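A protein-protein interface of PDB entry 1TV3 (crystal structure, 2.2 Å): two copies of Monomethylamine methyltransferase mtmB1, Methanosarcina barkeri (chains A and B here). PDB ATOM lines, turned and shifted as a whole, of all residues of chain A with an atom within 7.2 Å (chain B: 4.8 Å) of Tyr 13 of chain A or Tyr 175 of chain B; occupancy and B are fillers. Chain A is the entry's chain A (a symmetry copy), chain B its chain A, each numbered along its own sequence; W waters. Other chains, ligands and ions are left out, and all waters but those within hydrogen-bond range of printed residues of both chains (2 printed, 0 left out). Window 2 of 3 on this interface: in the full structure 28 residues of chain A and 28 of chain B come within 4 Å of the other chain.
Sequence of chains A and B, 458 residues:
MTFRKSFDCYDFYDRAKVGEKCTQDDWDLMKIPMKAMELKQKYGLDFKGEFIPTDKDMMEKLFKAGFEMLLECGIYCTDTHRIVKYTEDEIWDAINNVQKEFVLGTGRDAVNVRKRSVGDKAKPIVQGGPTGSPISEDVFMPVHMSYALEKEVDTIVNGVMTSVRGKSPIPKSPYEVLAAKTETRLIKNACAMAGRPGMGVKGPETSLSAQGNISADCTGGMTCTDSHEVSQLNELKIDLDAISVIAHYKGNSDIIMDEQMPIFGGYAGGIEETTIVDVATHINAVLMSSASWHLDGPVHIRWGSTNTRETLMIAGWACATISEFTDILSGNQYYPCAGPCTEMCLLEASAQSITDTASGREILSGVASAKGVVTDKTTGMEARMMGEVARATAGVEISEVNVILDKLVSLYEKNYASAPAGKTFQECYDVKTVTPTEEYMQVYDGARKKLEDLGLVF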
ATOM      1  N   ARG A   4      -0.695 -33.492 -12.040  1.00  0.00           N
ATOM      2  CA  ARG A   4      -2.144 -33.567 -12.187  1.00  0.00           C
ATOM      3  C   ARG A   4      -2.563 -32.881 -13.485  1.00  0.00           C
ATOM      4  O   ARG A   4      -3.306 -33.445 -14.286  1.00  0.00           O
ATOM      5  CB  ARG A   4      -2.838 -32.908 -10.990  1.00  0.00           C
ATOM      6  CG  ARG A   4      -4.323 -33.229 -10.902  1.00  0.00           C
ATOM      7  CD  ARG A   4      -5.004 -32.536  -9.728  1.00  0.00           C
ATOM      8  NE  ARG A   4      -4.905 -31.081  -9.821  1.00  0.00           N
ATOM      9  CZ  ARG A   4      -5.875 -30.238  -9.470  1.00  0.00           C
ATOM     10  NH1 ARG A   4      -7.027 -30.699  -9.000  1.00  0.00           N
ATOM     11  NH2 ARG A   4      -5.693 -28.930  -9.595  1.00  0.00           N
ATOM     12  N   PHE A   7       0.748 -26.856 -15.095  1.00  0.00           N
ATOM     13  CA  PHE A   7       0.607 -25.712 -14.201  1.00  0.00           C
ATOM     14  C   PHE A   7       0.343 -24.384 -14.913  1.00  0.00           C
ATOM     15  O   PHE A   7       0.980 -24.067 -15.923  1.00  0.00           O
ATOM     16  CB  PHE A   7       1.867 -25.570 -13.337  1.00  0.00           C
ATOM     17  CG  PHE A   7       1.738 -24.546 -12.241  1.00  0.00           C
ATOM     18  CD1 PHE A   7       1.314 -24.916 -10.971  1.00  0.00           C
ATOM     19  CD2 PHE A   7       2.013 -23.204 -12.491  1.00  0.00           C
ATOM     20  CE1 PHE A   7       1.160 -23.967  -9.963  1.00  0.00           C
ATOM     21  CE2 PHE A   7       1.862 -22.245 -11.490  1.00  0.00           C
ATOM     22  CZ  PHE A   7       1.435 -22.629 -10.223  1.00  0.00           C
ATOM     23  N   ASP A   8      -0.593 -23.608 -14.374  1.00  0.00           N
ATOM     24  CA  ASP A   8      -0.918 -22.300 -14.934  1.00  0.00           C
ATOM     25  C   ASP A   8      -1.256 -21.295 -13.831  1.00  0.00           C
ATOM     26  O   ASP A   8      -1.281 -21.634 -12.645  1.00  0.00           O
ATOM     27  CB  ASP A   8      -2.083 -22.392 -15.935  1.00  0.00           C
ATOM     28  CG  ASP A   8      -3.355 -22.933 -15.314  1.00  0.00           C
ATOM     29  OD1 ASP A   8      -3.630 -22.606 -14.139  1.00  0.00           O
ATOM     30  OD2 ASP A   8      -4.090 -23.674 -16.009  1.00  0.00           O
ATOM     31  N   CYS A   9      -1.518 -20.059 -14.236  1.00  0.00           N
ATOM     32  CA  CYS A   9      -1.838 -18.988 -13.304  1.00  0.00           C
ATOM     33  C   CYS A   9      -3.015 -19.325 -12.385  1.00  0.00           C
ATOM     34  O   CYS A   9      -3.106 -18.805 -11.273  1.00  0.00           O
ATOM     35  CB  CYS A   9      -2.131 -17.698 -14.078  1.00  0.00           C
ATOM     36  SG  CYS A   9      -3.444 -17.864 -15.314  1.00  0.00           S
ATOM     37  N   TYR A  10      -3.917 -20.189 -12.843  1.00  0.00           N
ATOM     38  CA  TYR A  10      -5.066 -20.560 -12.023  1.00  0.00           C
ATOM     39  C   TYR A  10      -4.635 -21.461 -10.870  1.00  0.00           C
ATOM     40  O   TYR A  10      -5.116 -21.310  -9.747  1.00  0.00           O
ATOM     41  CB  TYR A  10      -6.131 -21.251 -12.877  1.00  0.00           C
ATOM     42  CG  TYR A  10      -6.581 -20.391 -14.033  1.00  0.00           C
ATOM     43  CD1 TYR A  10      -6.092 -20.611 -15.323  1.00  0.00           C
ATOM     44  CD2 TYR A  10      -7.436 -19.311 -13.825  1.00  0.00           C
ATOM     45  CE1 TYR A  10      -6.440 -19.767 -16.378  1.00  0.00           C
ATOM     46  CE2 TYR A  10      -7.793 -18.460 -14.870  1.00  0.00           C
ATOM     47  CZ  TYR A  10      -7.290 -18.692 -16.143  1.00  0.00           C
ATOM     48  OH  TYR A  10      -7.633 -17.849 -17.173  1.00  0.00           O
ATOM     49  N   ASP A  11      -3.731 -22.395 -11.149  1.00  0.00           N
ATOM     50  CA  ASP A  11      -3.224 -23.284 -10.110  1.00  0.00           C
ATOM     51  C   ASP A  11      -2.456 -22.432  -9.103  1.00  0.00           C
ATOM     52  O   ASP A  11      -2.537 -22.658  -7.896  1.00  0.00           O
ATOM     53  CB  ASP A  11      -2.276 -24.332 -10.698  1.00  0.00           C
ATOM     54  CG  ASP A  11      -2.951 -25.227 -11.711  1.00  0.00           C
ATOM     55  OD1 ASP A  11      -4.029 -25.769 -11.397  1.00  0.00           O
ATOM     56  OD2 ASP A  11      -2.402 -25.399 -12.820  1.00  0.00           O
ATOM     57  N   PHE A  12      -1.711 -21.449  -9.603  1.00  0.00           N
ATOM     58  CA  PHE A  12      -0.937 -20.586  -8.724  1.00  0.00           C
ATOM     59  C   PHE A  12      -1.839 -19.892  -7.716  1.00  0.00           C
ATOM     60  O   PHE A  12      -1.545 -19.878  -6.521  1.00  0.00           O
ATOM     61  CB  PHE A  12      -0.175 -19.521  -9.508  1.00  0.00           C
ATOM     62  CG  PHE A  12       0.872 -18.826  -8.687  1.00  0.00           C
ATOM     63  CD1 PHE A  12       2.179 -19.302  -8.662  1.00  0.00           C
ATOM     64  CD2 PHE A  12       0.534 -17.746  -7.874  1.00  0.00           C
ATOM     65  CE1 PHE A  12       3.136 -18.720  -7.832  1.00  0.00           C
ATOM     66  CE2 PHE A  12       1.481 -17.157  -7.040  1.00  0.00           C
ATOM     67  CZ  PHE A  12       2.786 -17.645  -7.017  1.00  0.00           C
ATOM     68  N   TYR A  13      -2.928 -19.303  -8.205  1.00  0.00           N
ATOM     69  CA  TYR A  13      -3.877 -18.609  -7.340  1.00  0.00           C
ATOM     70  C   TYR A  13      -4.392 -19.575  -6.278  1.00  0.00           C
ATOM     71  O   TYR A  13      -4.405 -19.258  -5.087  1.00  0.00           O
ATOM     72  CB  TYR A  13      -5.059 -18.078  -8.154  1.00  0.00           C
ATOM     73  CG  TYR A  13      -6.128 -17.415  -7.309  1.00  0.00           C
ATOM     74  CD1 TYR A  13      -5.949 -16.127  -6.808  1.00  0.00           C
ATOM     75  CD2 TYR A  13      -7.306 -18.088  -6.982  1.00  0.00           C
ATOM     76  CE1 TYR A  13      -6.915 -15.522  -6.003  1.00  0.00           C
ATOM     77  CE2 TYR A  13      -8.279 -17.495  -6.178  1.00  0.00           C
ATOM     78  CZ  TYR A  13      -8.077 -16.213  -5.692  1.00  0.00           C
ATOM     79  OH  TYR A  13      -9.033 -15.620  -4.899  1.00  0.00           O
ATOM     80  N   ASP A  14      -4.826 -20.752  -6.722  1.00  0.00           N
ATOM     81  CA  ASP A  14      -5.336 -21.769  -5.813  1.00  0.00           C
ATOM     82  C   ASP A  14      -4.332 -22.028  -4.688  1.00  0.00           C
ATOM     83  O   ASP A  14      -4.659 -21.920  -3.504  1.00  0.00           O
ATOM     84  CB  ASP A  14      -5.590 -23.082  -6.569  1.00  0.00           C
ATOM     85  CG  ASP A  14      -6.770 -23.001  -7.529  1.00  0.00           C
ATOM     86  OD1 ASP A  14      -6.957 -23.962  -8.306  1.00  0.00           O
ATOM     87  OD2 ASP A  14      -7.514 -21.996  -7.507  1.00  0.00           O
ATOM     88  N   ARG A  15      -3.102 -22.357  -5.068  1.00  0.00           N
ATOM     89  CA  ARG A  15      -2.057 -22.660  -4.098  1.00  0.00           C
ATOM     90  C   ARG A  15      -1.636 -21.480  -3.228  1.00  0.00           C
ATOM     91  O   ARG A  15      -1.272 -21.662  -2.066  1.00  0.00           O
ATOM     92  CB  ARG A  15      -0.843 -23.247  -4.823  1.00  0.00           C
ATOM     93  CG  ARG A  15      -1.192 -24.503  -5.608  1.00  0.00           C
ATOM     94  CD  ARG A  15       0.006 -25.134  -6.300  1.00  0.00           C
ATOM     95  NE  ARG A  15      -0.437 -26.209  -7.190  1.00  0.00           N
ATOM     96  CZ  ARG A  15       0.369 -27.034  -7.849  1.00  0.00           C
ATOM     97  NH1 ARG A  15       1.688 -26.930  -7.728  1.00  0.00           N
ATOM     98  NH2 ARG A  15      -0.151 -27.957  -8.646  1.00  0.00           N
ATOM     99  N   ALA A  16      -1.695 -20.274  -3.781  1.00  0.00           N
ATOM    100  CA  ALA A  16      -1.306 -19.083  -3.039  1.00  0.00           C
ATOM    101  C   ALA A  16      -2.244 -18.802  -1.864  1.00  0.00           C
ATOM    102  O   ALA A  16      -1.866 -18.107  -0.919  1.00  0.00           O
ATOM    103  CB  ALA A  16      -1.265 -17.876  -3.968  1.00  0.00           C
ATOM    104  N   LYS A  17      -3.460 -19.342  -1.914  1.00  0.00           N
ATOM    105  CA  LYS A  17      -4.421 -19.108  -0.843  1.00  0.00           C
ATOM    106  C   LYS A  17      -4.285 -20.099   0.309  1.00  0.00           C
ATOM    107  O   LYS A  17      -4.688 -19.800   1.431  1.00  0.00           O
ATOM    108  CB  LYS A  17      -5.854 -19.161  -1.384  1.00  0.00           C
ATOM    109  CG  LYS A  17      -6.115 -18.239  -2.569  1.00  0.00           C
ATOM    110  CD  LYS A  17      -6.224 -16.762  -2.189  1.00  0.00           C
ATOM    111  CE  LYS A  17      -7.618 -16.463  -1.639  1.00  0.00           C
ATOM    112  NZ  LYS A  17      -8.645 -17.114  -2.525  1.00  0.00           N
ATOM    113  N   VAL A  18      -3.713 -21.270   0.046  1.00  0.00           N
ATOM    114  CA  VAL A  18      -3.578 -22.282   1.089  1.00  0.00           C
ATOM    115  C   VAL A  18      -2.152 -22.759   1.338  1.00  0.00           C
ATOM    116  O   VAL A  18      -1.937 -23.736   2.057  1.00  0.00           O
ATOM    117  CB  VAL A  18      -4.458 -23.508   0.760  1.00  0.00           C
ATOM    118  CG1 VAL A  18      -5.911 -23.072   0.606  1.00  0.00           C
ATOM    119  CG2 VAL A  18      -3.967 -24.181  -0.513  1.00  0.00           C
ATOM    120  N   CYS A  77       3.972 -15.421  -2.532  1.00  0.00           N
ATOM    121  CA  CYS A  77       2.886 -14.560  -2.993  1.00  0.00           C
ATOM    122  C   CYS A  77       2.708 -13.439  -1.970  1.00  0.00           C
ATOM    123  O   CYS A  77       2.253 -13.675  -0.849  1.00  0.00           O
ATOM    124  CB  CYS A  77       1.581 -15.347  -3.125  1.00  0.00           C
ATOM    125  SG  CYS A  77       0.195 -14.313  -3.670  1.00  0.00           S
ATOM    126  N   THR A  80      -1.054 -12.893  -0.298  1.00  0.00           N
ATOM    127  CA  THR A  80      -1.517 -13.872   0.679  1.00  0.00           C
ATOM    128  C   THR A  80      -0.468 -14.224   1.728  1.00  0.00           C
ATOM    129  O   THR A  80      -0.776 -14.883   2.719  1.00  0.00           O
ATOM    130  CB  THR A  80      -1.949 -15.175  -0.019  1.00  0.00           C
ATOM    131  OG1 THR A  80      -0.821 -15.744  -0.697  1.00  0.00           O
ATOM    132  CG2 THR A  80      -3.061 -14.902  -1.027  1.00  0.00           C
ATOM    133  N   VAL A  84       3.965 -20.841  -2.707  1.00  0.00           N
ATOM    134  CA  VAL A  84       3.423 -21.775  -3.691  1.00  0.00           C
ATOM    135  C   VAL A  84       4.550 -22.721  -4.074  1.00  0.00           C
ATOM    136  O   VAL A  84       5.640 -22.282  -4.442  1.00  0.00           O
ATOM    137  CB  VAL A  84       2.925 -21.051  -4.965  1.00  0.00           C
ATOM    138  CG1 VAL A  84       2.569 -22.075  -6.042  1.00  0.00           C
ATOM    139  CG2 VAL A  84       1.712 -20.193  -4.634  1.00  0.00           C
ATOM    140  N   LEU A 240      -0.684 -11.000  -6.818  1.00  0.00           N
ATOM    141  CA  LEU A 240      -1.864 -11.520  -7.499  1.00  0.00           C
ATOM    142  C   LEU A 240      -2.323 -10.696  -8.701  1.00  0.00           C
ATOM    143  O   LEU A 240      -2.931 -11.238  -9.622  1.00  0.00           O
ATOM    144  CB  LEU A 240      -3.011 -11.700  -6.499  1.00  0.00           C
ATOM    145  CG  LEU A 240      -2.769 -12.800  -5.457  1.00  0.00           C
ATOM    146  CD1 LEU A 240      -4.008 -12.968  -4.594  1.00  0.00           C
ATOM    147  CD2 LEU A 240      -2.428 -14.115  -6.147  1.00  0.00           C
ATOM    148  N   ILE A 243      -0.951 -12.135 -11.648  1.00  0.00           N
ATOM    149  CA  ILE A 243      -1.593 -13.411 -11.946  1.00  0.00           C
ATOM    150  C   ILE A 243      -2.855 -13.210 -12.795  1.00  0.00           C
ATOM    151  O   ILE A 243      -3.123 -13.989 -13.714  1.00  0.00           O
ATOM    152  CB  ILE A 243      -1.945 -14.166 -10.638  1.00  0.00           C
ATOM    153  CG1 ILE A 243      -0.657 -14.505  -9.872  1.00  0.00           C
ATOM    154  CG2 ILE A 243      -2.747 -15.425 -10.950  1.00  0.00           C
ATOM    155  CD1 ILE A 243       0.347 -15.349 -10.655  1.00  0.00           C
ATOM    156  N   SER A 244      -3.627 -12.170 -12.486  1.00  0.00           N
ATOM    157  CA  SER A 244      -4.837 -11.872 -13.249  1.00  0.00           C
ATOM    158  C   SER A 244      -4.486 -11.356 -14.644  1.00  0.00           C
ATOM    159  O   SER A 244      -5.161 -11.682 -15.622  1.00  0.00           O
ATOM    160  CB  SER A 244      -5.700 -10.837 -12.525  1.00  0.00           C
ATOM    161  OG  SER A 244      -6.471 -11.444 -11.505  1.00  0.00           O
ATOM    162  N   ALA A 247      -3.750 -14.200 -16.899  1.00  0.00           N
ATOM    163  CA  ALA A 247      -4.969 -14.870 -17.341  1.00  0.00           C
ATOM    164  C   ALA A 247      -5.576 -14.133 -18.533  1.00  0.00           C
ATOM    165  O   ALA A 247      -6.116 -14.748 -19.451  1.00  0.00           O
ATOM    166  CB  ALA A 247      -5.980 -14.943 -16.195  1.00  0.00           C
ATOM    167  N   VAL B 164     -16.351 -21.452 -13.139  1.00  0.00           N
ATOM    168  CA  VAL B 164     -15.718 -21.603 -14.437  1.00  0.00           C
ATOM    169  C   VAL B 164     -14.568 -22.573 -14.189  1.00  0.00           C
ATOM    170  O   VAL B 164     -13.726 -22.353 -13.315  1.00  0.00           O
ATOM    171  CB  VAL B 164     -15.243 -20.235 -14.996  1.00  0.00           C
ATOM    172  CG1 VAL B 164     -14.194 -19.620 -14.092  1.00  0.00           C
ATOM    173  CG2 VAL B 164     -14.732 -20.411 -16.418  1.00  0.00           C
ATOM    174  N   LYS B 167     -14.391 -23.572 -10.572  1.00  0.00           N
ATOM    175  CA  LYS B 167     -13.934 -22.651  -9.532  1.00  0.00           C
ATOM    176  C   LYS B 167     -14.780 -21.387  -9.507  1.00  0.00           C
ATOM    177  O   LYS B 167     -15.277 -20.953 -10.543  1.00  0.00           O
ATOM    178  CB  LYS B 167     -12.476 -22.265  -9.784  1.00  0.00           C
ATOM    179  CG  LYS B 167     -11.502 -23.427  -9.741  1.00  0.00           C
ATOM    180  CD  LYS B 167     -11.329 -23.937  -8.326  1.00  0.00           C
ATOM    181  CE  LYS B 167     -10.245 -24.990  -8.256  1.00  0.00           C
ATOM    182  NZ  LYS B 167     -10.028 -25.409  -6.847  1.00  0.00           N
ATOM    183  N   SER B 168     -14.934 -20.794  -8.326  1.00  0.00           N
ATOM    184  CA  SER B 168     -15.708 -19.566  -8.190  1.00  0.00           C
ATOM    185  C   SER B 168     -14.923 -18.411  -8.793  1.00  0.00           C
ATOM    186  O   SER B 168     -13.734 -18.262  -8.528  1.00  0.00           O
ATOM    187  CB  SER B 168     -15.992 -19.264  -6.717  1.00  0.00           C
ATOM    188  OG  SER B 168     -16.808 -20.264  -6.139  1.00  0.00           O
ATOM    189  N   PRO B 169     -15.579 -17.578  -9.616  1.00  0.00           N
ATOM    190  CA  PRO B 169     -14.920 -16.431 -10.248  1.00  0.00           C
ATOM    191  C   PRO B 169     -14.698 -15.295  -9.250  1.00  0.00           C
ATOM    192  O   PRO B 169     -15.164 -14.171  -9.453  1.00  0.00           O
ATOM    193  CB  PRO B 169     -15.898 -16.049 -11.354  1.00  0.00           C
ATOM    194  CG  PRO B 169     -17.221 -16.354 -10.728  1.00  0.00           C
ATOM    195  CD  PRO B 169     -16.975 -17.700 -10.074  1.00  0.00           C
ATOM    196  N   ILE B 170     -13.982 -15.600  -8.173  1.00  0.00           N
ATOM    197  CA  ILE B 170     -13.709 -14.623  -7.124  1.00  0.00           C
ATOM    198  C   ILE B 170     -13.152 -13.311  -7.667  1.00  0.00           C
ATOM    199  O   ILE B 170     -12.205 -13.298  -8.452  1.00  0.00           O
ATOM    200  CB  ILE B 170     -12.726 -15.200  -6.083  1.00  0.00           C
ATOM    201  CG1 ILE B 170     -13.315 -16.480  -5.485  1.00  0.00           C
ATOM    202  CG2 ILE B 170     -12.450 -14.172  -4.988  1.00  0.00           C
ATOM    203  CD1 ILE B 170     -12.391 -17.195  -4.523  1.00  0.00           C
ATOM    204  N   SER B 173      -9.403 -12.307  -8.922  1.00  0.00           N
ATOM    205  CA  SER B 173      -8.664 -13.561  -9.020  1.00  0.00           C
ATOM    206  C   SER B 173      -8.588 -13.832 -10.522  1.00  0.00           C
ATOM    207  O   SER B 173      -9.354 -13.257 -11.296  1.00  0.00           O
ATOM    208  CB  SER B 173      -9.428 -14.705  -8.350  1.00  0.00           C
ATOM    209  OG  SER B 173     -10.499 -15.144  -9.176  1.00  0.00           O
ATOM    210  N   PRO B 174      -7.663 -14.697 -10.960  1.00  0.00           N
ATOM    211  CA  PRO B 174      -7.591 -14.965 -12.400  1.00  0.00           C
ATOM    212  C   PRO B 174      -8.885 -15.586 -12.935  1.00  0.00           C
ATOM    213  O   PRO B 174      -9.207 -15.443 -14.114  1.00  0.00           O
ATOM    214  CB  PRO B 174      -6.385 -15.901 -12.522  1.00  0.00           C
ATOM    215  CG  PRO B 174      -6.338 -16.588 -11.166  1.00  0.00           C
ATOM    216  CD  PRO B 174      -6.615 -15.430 -10.231  1.00  0.00           C
ATOM    217  N   TYR B 175      -9.630 -16.267 -12.068  1.00  0.00           N
ATOM    218  CA  TYR B 175     -10.883 -16.886 -12.482  1.00  0.00           C
ATOM    219  C   TYR B 175     -11.931 -15.849 -12.879  1.00  0.00           C
ATOM    220  O   TYR B 175     -12.803 -16.126 -13.704  1.00  0.00           O
ATOM    221  CB  TYR B 175     -11.443 -17.782 -11.371  1.00  0.00           C
ATOM    222  CG  TYR B 175     -10.608 -19.009 -11.105  1.00  0.00           C
ATOM    223  CD1 TYR B 175      -9.786 -19.088  -9.983  1.00  0.00           C
ATOM    224  CD2 TYR B 175     -10.625 -20.089 -11.989  1.00  0.00           C
ATOM    225  CE1 TYR B 175      -8.998 -20.216  -9.742  1.00  0.00           C
ATOM    226  CE2 TYR B 175      -9.840 -21.220 -11.760  1.00  0.00           C
ATOM    227  CZ  TYR B 175      -9.033 -21.276 -10.633  1.00  0.00           C
ATOM    228  OH  TYR B 175      -8.273 -22.392 -10.388  1.00  0.00           O
ATOM    229  N   GLU B 176     -11.859 -14.658 -12.290  1.00  0.00           N
ATOM    230  CA  GLU B 176     -12.816 -13.616 -12.636  1.00  0.00           C
ATOM    231  C   GLU B 176     -12.575 -13.187 -14.083  1.00  0.00           C
ATOM    232  O   GLU B 176     -13.523 -12.968 -14.835  1.00  0.00           O
ATOM    233  CB  GLU B 176     -12.682 -12.401 -11.711  1.00  0.00           C
ATOM    234  CG  GLU B 176     -13.604 -11.259 -12.130  1.00  0.00           C
ATOM    235  CD  GLU B 176     -13.413  -9.994 -11.317  1.00  0.00           C
ATOM    236  OE1 GLU B 176     -12.248  -9.639 -11.023  1.00  0.00           O
ATOM    237  OE2 GLU B 176     -14.433  -9.346 -10.994  1.00  0.00           O
ATOM    238  N   VAL B 177     -11.303 -13.062 -14.460  1.00  0.00           N
ATOM    239  CA  VAL B 177     -10.940 -12.682 -15.824  1.00  0.00           C
ATOM    240  C   VAL B 177     -11.383 -13.782 -16.786  1.00  0.00           C
ATOM    241  O   VAL B 177     -11.975 -13.500 -17.827  1.00  0.00           O
ATOM    242  CB  VAL B 177      -9.405 -12.464 -15.960  1.00  0.00           C
ATOM    243  CG1 VAL B 177      -8.987 -12.474 -17.429  1.00  0.00           C
ATOM    244  CG2 VAL B 177      -9.022 -11.138 -15.325  1.00  0.00           C
ATOM    245  N   LEU B 178     -11.104 -15.033 -16.432  1.00  0.00           N
ATOM    246  CA  LEU B 178     -11.493 -16.162 -17.274  1.00  0.00           C
ATOM    247  C   LEU B 178     -13.003 -16.173 -17.509  1.00  0.00           C
ATOM    248  O   LEU B 178     -13.463 -16.385 -18.635  1.00  0.00           O
ATOM    249  CB  LEU B 178     -11.062 -17.484 -16.628  1.00  0.00           C
ATOM    250  CG  LEU B 178     -11.467 -18.772 -17.363  1.00  0.00           C
ATOM    251  CD1 LEU B 178     -10.878 -18.791 -18.779  1.00  0.00           C
ATOM    252  CD2 LEU B 178     -10.983 -19.983 -16.569  1.00  0.00           C
ATOM    253  N   ALA B 179     -13.770 -15.932 -16.447  1.00  0.00           N
ATOM    254  CA  ALA B 179     -15.227 -15.916 -16.538  1.00  0.00           C
ATOM    255  C   ALA B 179     -15.741 -14.745 -17.369  1.00  0.00           C
ATOM    256  O   ALA B 179     -16.715 -14.883 -18.113  1.00  0.00           O
ATOM    257  CB  ALA B 179     -15.841 -15.868 -15.138  1.00  0.00           C
HETATM  258  O   HOH W   1      -9.358 -22.886  -4.770  1.00  0.00           O
HETATM  259  O   HOH W   2      -9.554 -10.383 -11.762  1.00  0.00           O
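No position is printed for both chains.
Of the 20 printed residues of chain A, 7 touch a printed residue of chain B.
Hydrophobic or aromatic side chains of chain A that line the printed part of chain B: Tyr 10, Tyr 13, Ile 243 and Ala 247.
Along chain A the printed residues that touch a printed residue of chain B span positions 9 to 247.
Of the 12 printed residues of chain B, 7 touch a printed residue of chain A.
Among the printed residues, 16 pairs touch across the chains.
Water W2 lies within hydrogen-bond range of the side-chain carboxylate of Glu 176 of chain B (2.9 Å), the backbone carbonyl oxygen of Ser 173 of chain B (2.9 Å) and the side-chain hydroxyl of Ser 244 of chain A (3.3 Å).
Water W1 bridges the side-chain amino group (NZ) of Lys 167 of chain B and the side-chain carboxylate (OD2) of Asp 14 of chain A.
The backbone carbonyl oxygen (O) of Ile 170 of chain B lies within hydrogen-bond range of the side-chain hydroxyl (OG) of Ser 173 of chain B (2.6 Å).
The side-chain hydroxyl of Ser 173 of chain B lies close to the backbone NH of Tyr 175 of chain B.
OD1 of Asp 8 of chain A lies within hydrogen-bond range of N of Tyr 10 of chain A (2.8 Å).
OH of Tyr 13 of chain A sits at hydrogen-bond distance from NZ of Lys 17 of chain A, 2.8 Å away.
The backbone NH (N) of Glu 176 of chain B lies within hydrogen-bond range of the side-chain hydroxyl (OG) of Ser 173 of chain B (3.4 Å).
Tyr 10 of chain A touches Pro 174 of chain B.
Leu 178 of chain B touches Tyr 10 of chain A (CB to OH, 3.5 Å).
OH of Tyr 13 of chain A touches CG2 of Ile 170 of chain B, 3.7 Å away.
CZ of Tyr 13 of chain A touches CB of Ser 173 of chain B (3.3 Å).
CD1 of Tyr 13 of chain A touches CD of Pro 174 of chain B, at 3.6 Å.
Tyr 13 of chain A touches Tyr 175 of chain B.
Pro 174 of chain B touches Ile 243 of chain A (CG to CG2, 3.8 Å).
OG of Ser 244 of chain A touches N of Pro 174 of chain B, at 3.5 Å.
Val 177 of chain B touches Ser 244 of chain A (CG2 to O, 3.9 Å).
Val 177 of chain B touches Ala 247 of chain A (CG1 to C, 3.95 Å).
The backbone carbonyl oxygen of Ser 173 of chain B lies close to the side-chain hydroxyl of Ser 244 of chain A (3.4 Å).
OH of Tyr 175 of chain B sits at hydrogen-bond distance from O of Tyr 10 of chain A (3.4 Å).
NZ of Lys 167 of chain B lies within salt-bridge range of OD1 of Asp 14 of chain A (3.7 Å).
OH of Tyr 175 of chain B is in hydrogen-bond range of OD1 of Asp 14 of chain A (2.9 Å).
Tyr 175 of chain B touches just these residues of chain A: Tyr 10, Tyr 13 and Asp 14.
Of the printed residues of chain A, Lys 167 of chain B touches Asp 14 (3.4 Å).
Of the printed residues of chain A, Ser 173 of chain B touches Tyr 13 and Ser 244.
The nearest printed residue of chain B that does not touch Tyr 13 of chain A is Ser 168 of chain B (6.0 Å).
The nearest residue of chain A that does not touch Tyr 175 of chain B is Asp 11 of chain A (4.6 Å).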
